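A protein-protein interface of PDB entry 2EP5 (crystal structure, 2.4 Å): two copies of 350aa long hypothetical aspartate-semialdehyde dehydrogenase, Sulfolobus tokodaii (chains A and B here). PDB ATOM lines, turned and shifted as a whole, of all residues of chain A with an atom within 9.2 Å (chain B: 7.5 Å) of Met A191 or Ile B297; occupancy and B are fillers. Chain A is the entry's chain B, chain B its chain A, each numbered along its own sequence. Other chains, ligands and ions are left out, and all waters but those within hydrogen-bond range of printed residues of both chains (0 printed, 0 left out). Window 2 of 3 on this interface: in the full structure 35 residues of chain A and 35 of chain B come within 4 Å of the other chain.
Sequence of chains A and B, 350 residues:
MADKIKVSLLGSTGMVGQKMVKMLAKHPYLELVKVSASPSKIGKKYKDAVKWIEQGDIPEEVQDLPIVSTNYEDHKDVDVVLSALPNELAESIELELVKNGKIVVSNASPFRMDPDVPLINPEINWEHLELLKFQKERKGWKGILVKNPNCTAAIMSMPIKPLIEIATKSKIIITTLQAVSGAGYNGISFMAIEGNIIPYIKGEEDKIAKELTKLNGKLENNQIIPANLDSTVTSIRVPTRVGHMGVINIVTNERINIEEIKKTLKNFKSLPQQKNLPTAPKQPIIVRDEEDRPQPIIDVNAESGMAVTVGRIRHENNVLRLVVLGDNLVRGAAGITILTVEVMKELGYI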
ATOM      1  N   ILE A 188       1.617  38.317  17.201  1.00  0.00           N
ATOM      2  CA  ILE A 188       1.330  37.041  17.844  1.00  0.00           C
ATOM      3  C   ILE A 188       2.443  36.601  18.791  1.00  0.00           C
ATOM      4  O   ILE A 188       3.622  36.590  18.422  1.00  0.00           O
ATOM      5  CB  ILE A 188       1.088  35.952  16.772  1.00  0.00           C
ATOM      6  CG1 ILE A 188      -0.050  36.408  15.845  1.00  0.00           C
ATOM      7  CG2 ILE A 188       0.719  34.625  17.427  1.00  0.00           C
ATOM      8  CD1 ILE A 188      -0.147  35.635  14.550  1.00  0.00           C
ATOM      9  N   SER A 189       2.063  36.233  20.013  1.00  0.00           N
ATOM     10  CA  SER A 189       3.053  35.808  20.998  1.00  0.00           C
ATOM     11  C   SER A 189       3.517  34.385  20.737  1.00  0.00           C
ATOM     12  O   SER A 189       2.822  33.595  20.089  1.00  0.00           O
ATOM     13  CB  SER A 189       2.497  35.909  22.427  1.00  0.00           C
ATOM     14  OG  SER A 189       1.617  34.838  22.723  1.00  0.00           O
ATOM     15  N   PHE A 190       4.707  34.086  21.245  1.00  0.00           N
ATOM     16  CA  PHE A 190       5.336  32.776  21.122  1.00  0.00           C
ATOM     17  C   PHE A 190       4.492  31.684  21.784  1.00  0.00           C
ATOM     18  O   PHE A 190       4.369  30.581  21.263  1.00  0.00           O
ATOM     19  CB  PHE A 190       6.719  32.829  21.785  1.00  0.00           C
ATOM     20  CG  PHE A 190       7.420  31.504  21.858  1.00  0.00           C
ATOM     21  CD1 PHE A 190       8.010  30.945  20.725  1.00  0.00           C
ATOM     22  CD2 PHE A 190       7.498  30.817  23.062  1.00  0.00           C
ATOM     23  CE1 PHE A 190       8.671  29.716  20.793  1.00  0.00           C
ATOM     24  CE2 PHE A 190       8.158  29.583  23.140  1.00  0.00           C
ATOM     25  CZ  PHE A 190       8.745  29.034  21.998  1.00  0.00           C
ATOM     26  N   MET A 191       3.922  32.004  22.940  1.00  0.00           N
ATOM     27  CA  MET A 191       3.113  31.064  23.702  1.00  0.00           C
ATOM     28  C   MET A 191       1.810  30.705  22.985  1.00  0.00           C
ATOM     29  O   MET A 191       1.302  29.583  23.096  1.00  0.00           O
ATOM     30  CB  MET A 191       2.789  31.663  25.081  1.00  0.00           C
ATOM     31  CG  MET A 191       3.998  31.909  26.001  1.00  0.00           C
ATOM     32  SD  MET A 191       4.811  30.390  26.567  1.00  0.00           S
ATOM     33  CE  MET A 191       3.669  29.837  27.834  1.00  0.00           C
ATOM     34  N   ALA A 192       1.270  31.661  22.247  1.00  0.00           N
ATOM     35  CA  ALA A 192       0.018  31.438  21.555  1.00  0.00           C
ATOM     36  C   ALA A 192       0.120  30.570  20.308  1.00  0.00           C
ATOM     37  O   ALA A 192      -0.835  29.876  19.974  1.00  0.00           O
ATOM     38  CB  ALA A 192      -0.611  32.778  21.201  1.00  0.00           C
ATOM     39  N   ILE A 193       1.271  30.569  19.640  1.00  0.00           N
ATOM     40  CA  ILE A 193       1.375  29.818  18.393  1.00  0.00           C
ATOM     41  C   ILE A 193       2.366  28.659  18.254  1.00  0.00           C
ATOM     42  O   ILE A 193       2.056  27.686  17.565  1.00  0.00           O
ATOM     43  CB  ILE A 193       1.589  30.802  17.194  1.00  0.00           C
ATOM     44  CG1 ILE A 193       1.484  30.057  15.856  1.00  0.00           C
ATOM     45  CG2 ILE A 193       2.953  31.446  17.288  1.00  0.00           C
ATOM     46  CD1 ILE A 193       0.112  29.460  15.574  1.00  0.00           C
ATOM     47  N   GLU A 194       3.537  28.728  18.889  1.00  0.00           N
ATOM     48  CA  GLU A 194       4.502  27.636  18.740  1.00  0.00           C
ATOM     49  C   GLU A 194       3.906  26.274  19.095  1.00  0.00           C
ATOM     50  O   GLU A 194       3.229  26.118  20.114  1.00  0.00           O
ATOM     51  CB  GLU A 194       5.777  27.907  19.551  1.00  0.00           C
ATOM     52  CG  GLU A 194       5.702  27.650  21.041  1.00  0.00           C
ATOM     53  CD  GLU A 194       5.820  26.180  21.379  1.00  0.00           C
ATOM     54  OE1 GLU A 194       6.672  25.507  20.755  1.00  0.00           O
ATOM     55  OE2 GLU A 194       5.070  25.710  22.271  1.00  0.00           O
ATOM     56  N   GLY A 195       4.151  25.301  18.218  1.00  0.00           N
ATOM     57  CA  GLY A 195       3.614  23.963  18.398  1.00  0.00           C
ATOM     58  C   GLY A 195       2.097  23.989  18.364  1.00  0.00           C
ATOM     59  O   GLY A 195       1.448  23.076  18.866  1.00  0.00           O
ATOM     60  N   ASN A 196       1.520  25.021  17.753  1.00  0.00           N
ATOM     61  CA  ASN A 196       0.064  25.136  17.725  1.00  0.00           C
ATOM     62  C   ASN A 196      -0.527  25.568  16.373  1.00  0.00           C
ATOM     63  O   ASN A 196       0.197  25.874  15.426  1.00  0.00           O
ATOM     64  CB  ASN A 196      -0.365  26.105  18.837  1.00  0.00           C
ATOM     65  CG  ASN A 196      -1.860  26.101  19.079  1.00  0.00           C
ATOM     66  OD1 ASN A 196      -2.491  25.046  19.106  1.00  0.00           O
ATOM     67  ND2 ASN A 196      -2.434  27.286  19.278  1.00  0.00           N
ATOM     68  N   ILE A 197      -1.855  25.577  16.293  1.00  0.00           N
ATOM     69  CA  ILE A 197      -2.568  25.970  15.082  1.00  0.00           C
ATOM     70  C   ILE A 197      -3.809  26.751  15.509  1.00  0.00           C
ATOM     71  O   ILE A 197      -4.507  26.335  16.425  1.00  0.00           O
ATOM     72  CB  ILE A 197      -3.034  24.720  14.272  1.00  0.00           C
ATOM     73  CG1 ILE A 197      -1.831  23.933  13.748  1.00  0.00           C
ATOM     74  CG2 ILE A 197      -3.910  25.138  13.113  1.00  0.00           C
ATOM     75  CD1 ILE A 197      -0.965  24.704  12.775  1.00  0.00           C
ATOM     76  N   ILE A 198      -4.078  27.884  14.864  1.00  0.00           N
ATOM     77  CA  ILE A 198      -5.278  28.665  15.175  1.00  0.00           C
ATOM     78  C   ILE A 198      -6.066  28.768  13.875  1.00  0.00           C
ATOM     79  O   ILE A 198      -5.759  29.582  13.004  1.00  0.00           O
ATOM     80  CB  ILE A 198      -4.951  30.075  15.706  1.00  0.00           C
ATOM     81  CG1 ILE A 198      -4.091  29.963  16.973  1.00  0.00           C
ATOM     82  CG2 ILE A 198      -6.271  30.827  15.995  1.00  0.00           C
ATOM     83  CD1 ILE A 198      -3.649  31.304  17.562  1.00  0.00           C
ATOM     84  N   PRO A 199      -7.108  27.939  13.741  1.00  0.00           N
ATOM     85  CA  PRO A 199      -8.000  27.832  12.584  1.00  0.00           C
ATOM     86  C   PRO A 199      -8.858  29.050  12.313  1.00  0.00           C
ATOM     87  O   PRO A 199     -10.001  28.915  11.894  1.00  0.00           O
ATOM     88  CB  PRO A 199      -8.841  26.613  12.933  1.00  0.00           C
ATOM     89  CG  PRO A 199      -9.073  26.831  14.390  1.00  0.00           C
ATOM     90  CD  PRO A 199      -7.681  27.216  14.895  1.00  0.00           C
ATOM     91  N   THR B 240       3.857  20.572  14.867  1.00  0.00           N
ATOM     92  CA  THR B 240       3.020  20.356  16.034  1.00  0.00           C
ATOM     93  C   THR B 240       3.441  19.014  16.629  1.00  0.00           C
ATOM     94  O   THR B 240       3.856  18.121  15.893  1.00  0.00           O
ATOM     95  CB  THR B 240       1.540  20.311  15.587  1.00  0.00           C
ATOM     96  OG1 THR B 240       1.061  21.652  15.426  1.00  0.00           O
ATOM     97  CG2 THR B 240       0.675  19.559  16.587  1.00  0.00           C
ATOM     98  N   VAL B 242       1.477  16.910  18.994  1.00  0.00           N
ATOM     99  CA  VAL B 242       0.366  15.977  18.986  1.00  0.00           C
ATOM    100  C   VAL B 242      -0.927  16.629  18.570  1.00  0.00           C
ATOM    101  O   VAL B 242      -1.212  17.763  18.960  1.00  0.00           O
ATOM    102  CB  VAL B 242       0.154  15.367  20.389  1.00  0.00           C
ATOM    103  CG1 VAL B 242      -0.912  14.267  20.323  1.00  0.00           C
ATOM    104  CG2 VAL B 242       1.482  14.836  20.929  1.00  0.00           C
ATOM    105  N   PRO B 294     -11.265  24.517  17.057  1.00  0.00           N
ATOM    106  CA  PRO B 294     -10.311  23.976  18.033  1.00  0.00           C
ATOM    107  C   PRO B 294      -8.850  24.337  17.779  1.00  0.00           C
ATOM    108  O   PRO B 294      -8.472  24.737  16.678  1.00  0.00           O
ATOM    109  CB  PRO B 294     -10.530  22.482  17.918  1.00  0.00           C
ATOM    110  CG  PRO B 294     -10.705  22.331  16.416  1.00  0.00           C
ATOM    111  CD  PRO B 294     -11.638  23.481  16.071  1.00  0.00           C
ATOM    112  N   GLN B 295      -8.040  24.182  18.821  1.00  0.00           N
ATOM    113  CA  GLN B 295      -6.610  24.442  18.760  1.00  0.00           C
ATOM    114  C   GLN B 295      -5.895  23.308  19.486  1.00  0.00           C
ATOM    115  O   GLN B 295      -6.279  22.925  20.587  1.00  0.00           O
ATOM    116  CB  GLN B 295      -6.254  25.761  19.457  1.00  0.00           C
ATOM    117  CG  GLN B 295      -6.593  27.027  18.704  1.00  0.00           C
ATOM    118  CD  GLN B 295      -6.133  28.256  19.460  1.00  0.00           C
ATOM    119  OE1 GLN B 295      -4.979  28.336  19.869  1.00  0.00           O
ATOM    120  NE2 GLN B 295      -7.033  29.218  19.654  1.00  0.00           N
ATOM    121  N   PRO B 296      -4.846  22.755  18.870  1.00  0.00           N
ATOM    122  CA  PRO B 296      -4.075  21.666  19.467  1.00  0.00           C
ATOM    123  C   PRO B 296      -3.733  21.846  20.951  1.00  0.00           C
ATOM    124  O   PRO B 296      -4.074  20.995  21.773  1.00  0.00           O
ATOM    125  CB  PRO B 296      -2.831  21.627  18.594  1.00  0.00           C
ATOM    126  CG  PRO B 296      -3.402  21.908  17.248  1.00  0.00           C
ATOM    127  CD  PRO B 296      -4.352  23.060  17.514  1.00  0.00           C
ATOM    128  N   ILE B 297      -3.076  22.955  21.300  1.00  0.00           N
ATOM    129  CA  ILE B 297      -2.671  23.176  22.689  1.00  0.00           C
ATOM    130  C   ILE B 297      -3.800  23.321  23.706  1.00  0.00           C
ATOM    131  O   ILE B 297      -3.563  23.216  24.907  1.00  0.00           O
ATOM    132  CB  ILE B 297      -1.717  24.397  22.832  1.00  0.00           C
ATOM    133  CG1 ILE B 297      -2.438  25.695  22.472  1.00  0.00           C
ATOM    134  CG2 ILE B 297      -0.506  24.204  21.946  1.00  0.00           C
ATOM    135  CD1 ILE B 297      -1.579  26.941  22.669  1.00  0.00           C
ATOM    136  N   ILE B 298      -5.022  23.542  23.236  1.00  0.00           N
ATOM    137  CA  ILE B 298      -6.155  23.697  24.141  1.00  0.00           C
ATOM    138  C   ILE B 298      -7.081  22.492  24.186  1.00  0.00           C
ATOM    139  O   ILE B 298      -7.506  22.072  25.258  1.00  0.00           O
ATOM    140  CB  ILE B 298      -7.053  24.900  23.751  1.00  0.00           C
ATOM    141  CG1 ILE B 298      -6.255  26.205  23.768  1.00  0.00           C
ATOM    142  CG2 ILE B 298      -8.247  24.988  24.708  1.00  0.00           C
ATOM    143  CD1 ILE B 298      -7.032  27.373  23.189  1.00  0.00           C
ATOM    144  N   ASP B 299      -7.385  21.935  23.018  1.00  0.00           N
ATOM    145  CA  ASP B 299      -8.335  20.836  22.916  1.00  0.00           C
ATOM    146  C   ASP B 299      -7.829  19.422  22.655  1.00  0.00           C
ATOM    147  O   ASP B 299      -8.595  18.468  22.755  1.00  0.00           O
ATOM    148  CB  ASP B 299      -9.363  21.202  21.847  1.00  0.00           C
ATOM    149  CG  ASP B 299     -10.017  22.546  22.108  1.00  0.00           C
ATOM    150  OD1 ASP B 299     -10.725  22.666  23.132  1.00  0.00           O
ATOM    151  OD2 ASP B 299      -9.822  23.481  21.296  1.00  0.00           O
ATOM    152  N   VAL B 300      -6.554  19.269  22.326  1.00  0.00           N
ATOM    153  CA  VAL B 300      -6.016  17.943  22.039  1.00  0.00           C
ATOM    154  C   VAL B 300      -6.277  16.898  23.125  1.00  0.00           C
ATOM    155  O   VAL B 300      -6.522  15.734  22.819  1.00  0.00           O
ATOM    156  CB  VAL B 300      -4.492  17.998  21.777  1.00  0.00           C
ATOM    157  CG1 VAL B 300      -3.732  18.162  23.081  1.00  0.00           C
ATOM    158  CG2 VAL B 300      -4.049  16.739  21.049  1.00  0.00           C
ATOM    159  N   ASN B 301      -6.236  17.310  24.386  1.00  0.00           N
ATOM    160  CA  ASN B 301      -6.435  16.381  25.494  1.00  0.00           C
ATOM    161  C   ASN B 301      -7.882  16.109  25.906  1.00  0.00           C
ATOM    162  O   ASN B 301      -8.123  15.355  26.847  1.00  0.00           O
ATOM    163  CB  ASN B 301      -5.645  16.860  26.718  1.00  0.00           C
ATOM    164  CG  ASN B 301      -4.150  16.870  26.478  1.00  0.00           C
ATOM    165  OD1 ASN B 301      -3.567  15.860  26.089  1.00  0.00           O
ATOM    166  ND2 ASN B 301      -3.516  18.015  26.711  1.00  0.00           N
ATOM    167  N   LEU B 325     -10.577  18.333  15.372  1.00  0.00           N
ATOM    168  CA  LEU B 325      -9.268  18.079  15.946  1.00  0.00           C
ATOM    169  C   LEU B 325      -9.360  16.851  16.835  1.00  0.00           C
ATOM    170  O   LEU B 325     -10.374  16.626  17.488  1.00  0.00           O
ATOM    171  CB  LEU B 325      -8.825  19.294  16.761  1.00  0.00           C
ATOM    172  CG  LEU B 325      -7.400  19.431  17.342  1.00  0.00           C
ATOM    173  CD1 LEU B 325      -7.416  19.182  18.832  1.00  0.00           C
ATOM    174  CD2 LEU B 325      -6.436  18.497  16.632  1.00  0.00           C
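N of Ile B297 is in hydrogen-bond range of OD1 of Asn A196, 3.1 Å away. The backbone nitrogen (N) of Pro B296 sits close to the side-chain amide oxygen (OD1) of Asn A196. The side-chain amide nitrogen (ND2) of Asn A196 sits at hydrogen-bond distance from the side-chain amide oxygen (OE1) of Gln B295 (2.8 Å).
The backbone NH (N) of Gln B295 lies within hydrogen-bond range of the side-chain carboxylate (OD2) of Asp B299, 3.1 Å away. O of Ala A192 is in hydrogen-bond range of ND2 of Asn A196, at 3.1 Å.
Ile B297 touches Met A191. Thr B240 touches Gly A195. O of Gly A195 touches CG2 of Ile B297 (3.8 Å). Ile A197 touches Gln B295 (O to CG, 3.2 Å). O of Ile A197 touches CD of Pro B296, 3.5 Å away. Gln B295 touches Ile A198. O of Pro B294 touches CD of Pro A199, 3.2 Å away. Gln B295 touches Pro A199.
Glu A194 touches none of the printed residues of chain B. Printed residues of chain B within 4 Å of Gly A195: Thr B240 and Ile B297. Of the printed residues of chain B, Asn A196 touches Gln B295, Pro B296 and Ile B297. Pro B296 touches two residues of chain A. Ile B297 touches just these residues of chain A: Met A191 (3.9 Å), Gly A195 (3.8 Å) and Asn A196 (3.1 Å). No residue of chain A comes within 4 Å of Ile B298. The nearest residue of chain A that does not touch Ile B297 is Ala A192 (4.1 Å).
Of the 12 printed residues of chain A, 6 touch a printed residue of chain B. Printed residues of chain A that touch a printed residue of chain B: Met A191, Gly A195, Asn A196, Ile A197, Ile A198 and Pro A199. Hydrophobic or aromatic side chains of chain A within 4 Å of the printed part of chain B: Ile A197, Ile A198 and Pro A199. Hydrophobic or aromatic side chains of chain B within 4 Å of the printed part of chain A: Pro B296 and Ile B297.
No position is printed for both chains. Of the 11 pairs that touch across the chains among the printed residues, none has its exchanged pair printed and touching as well.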
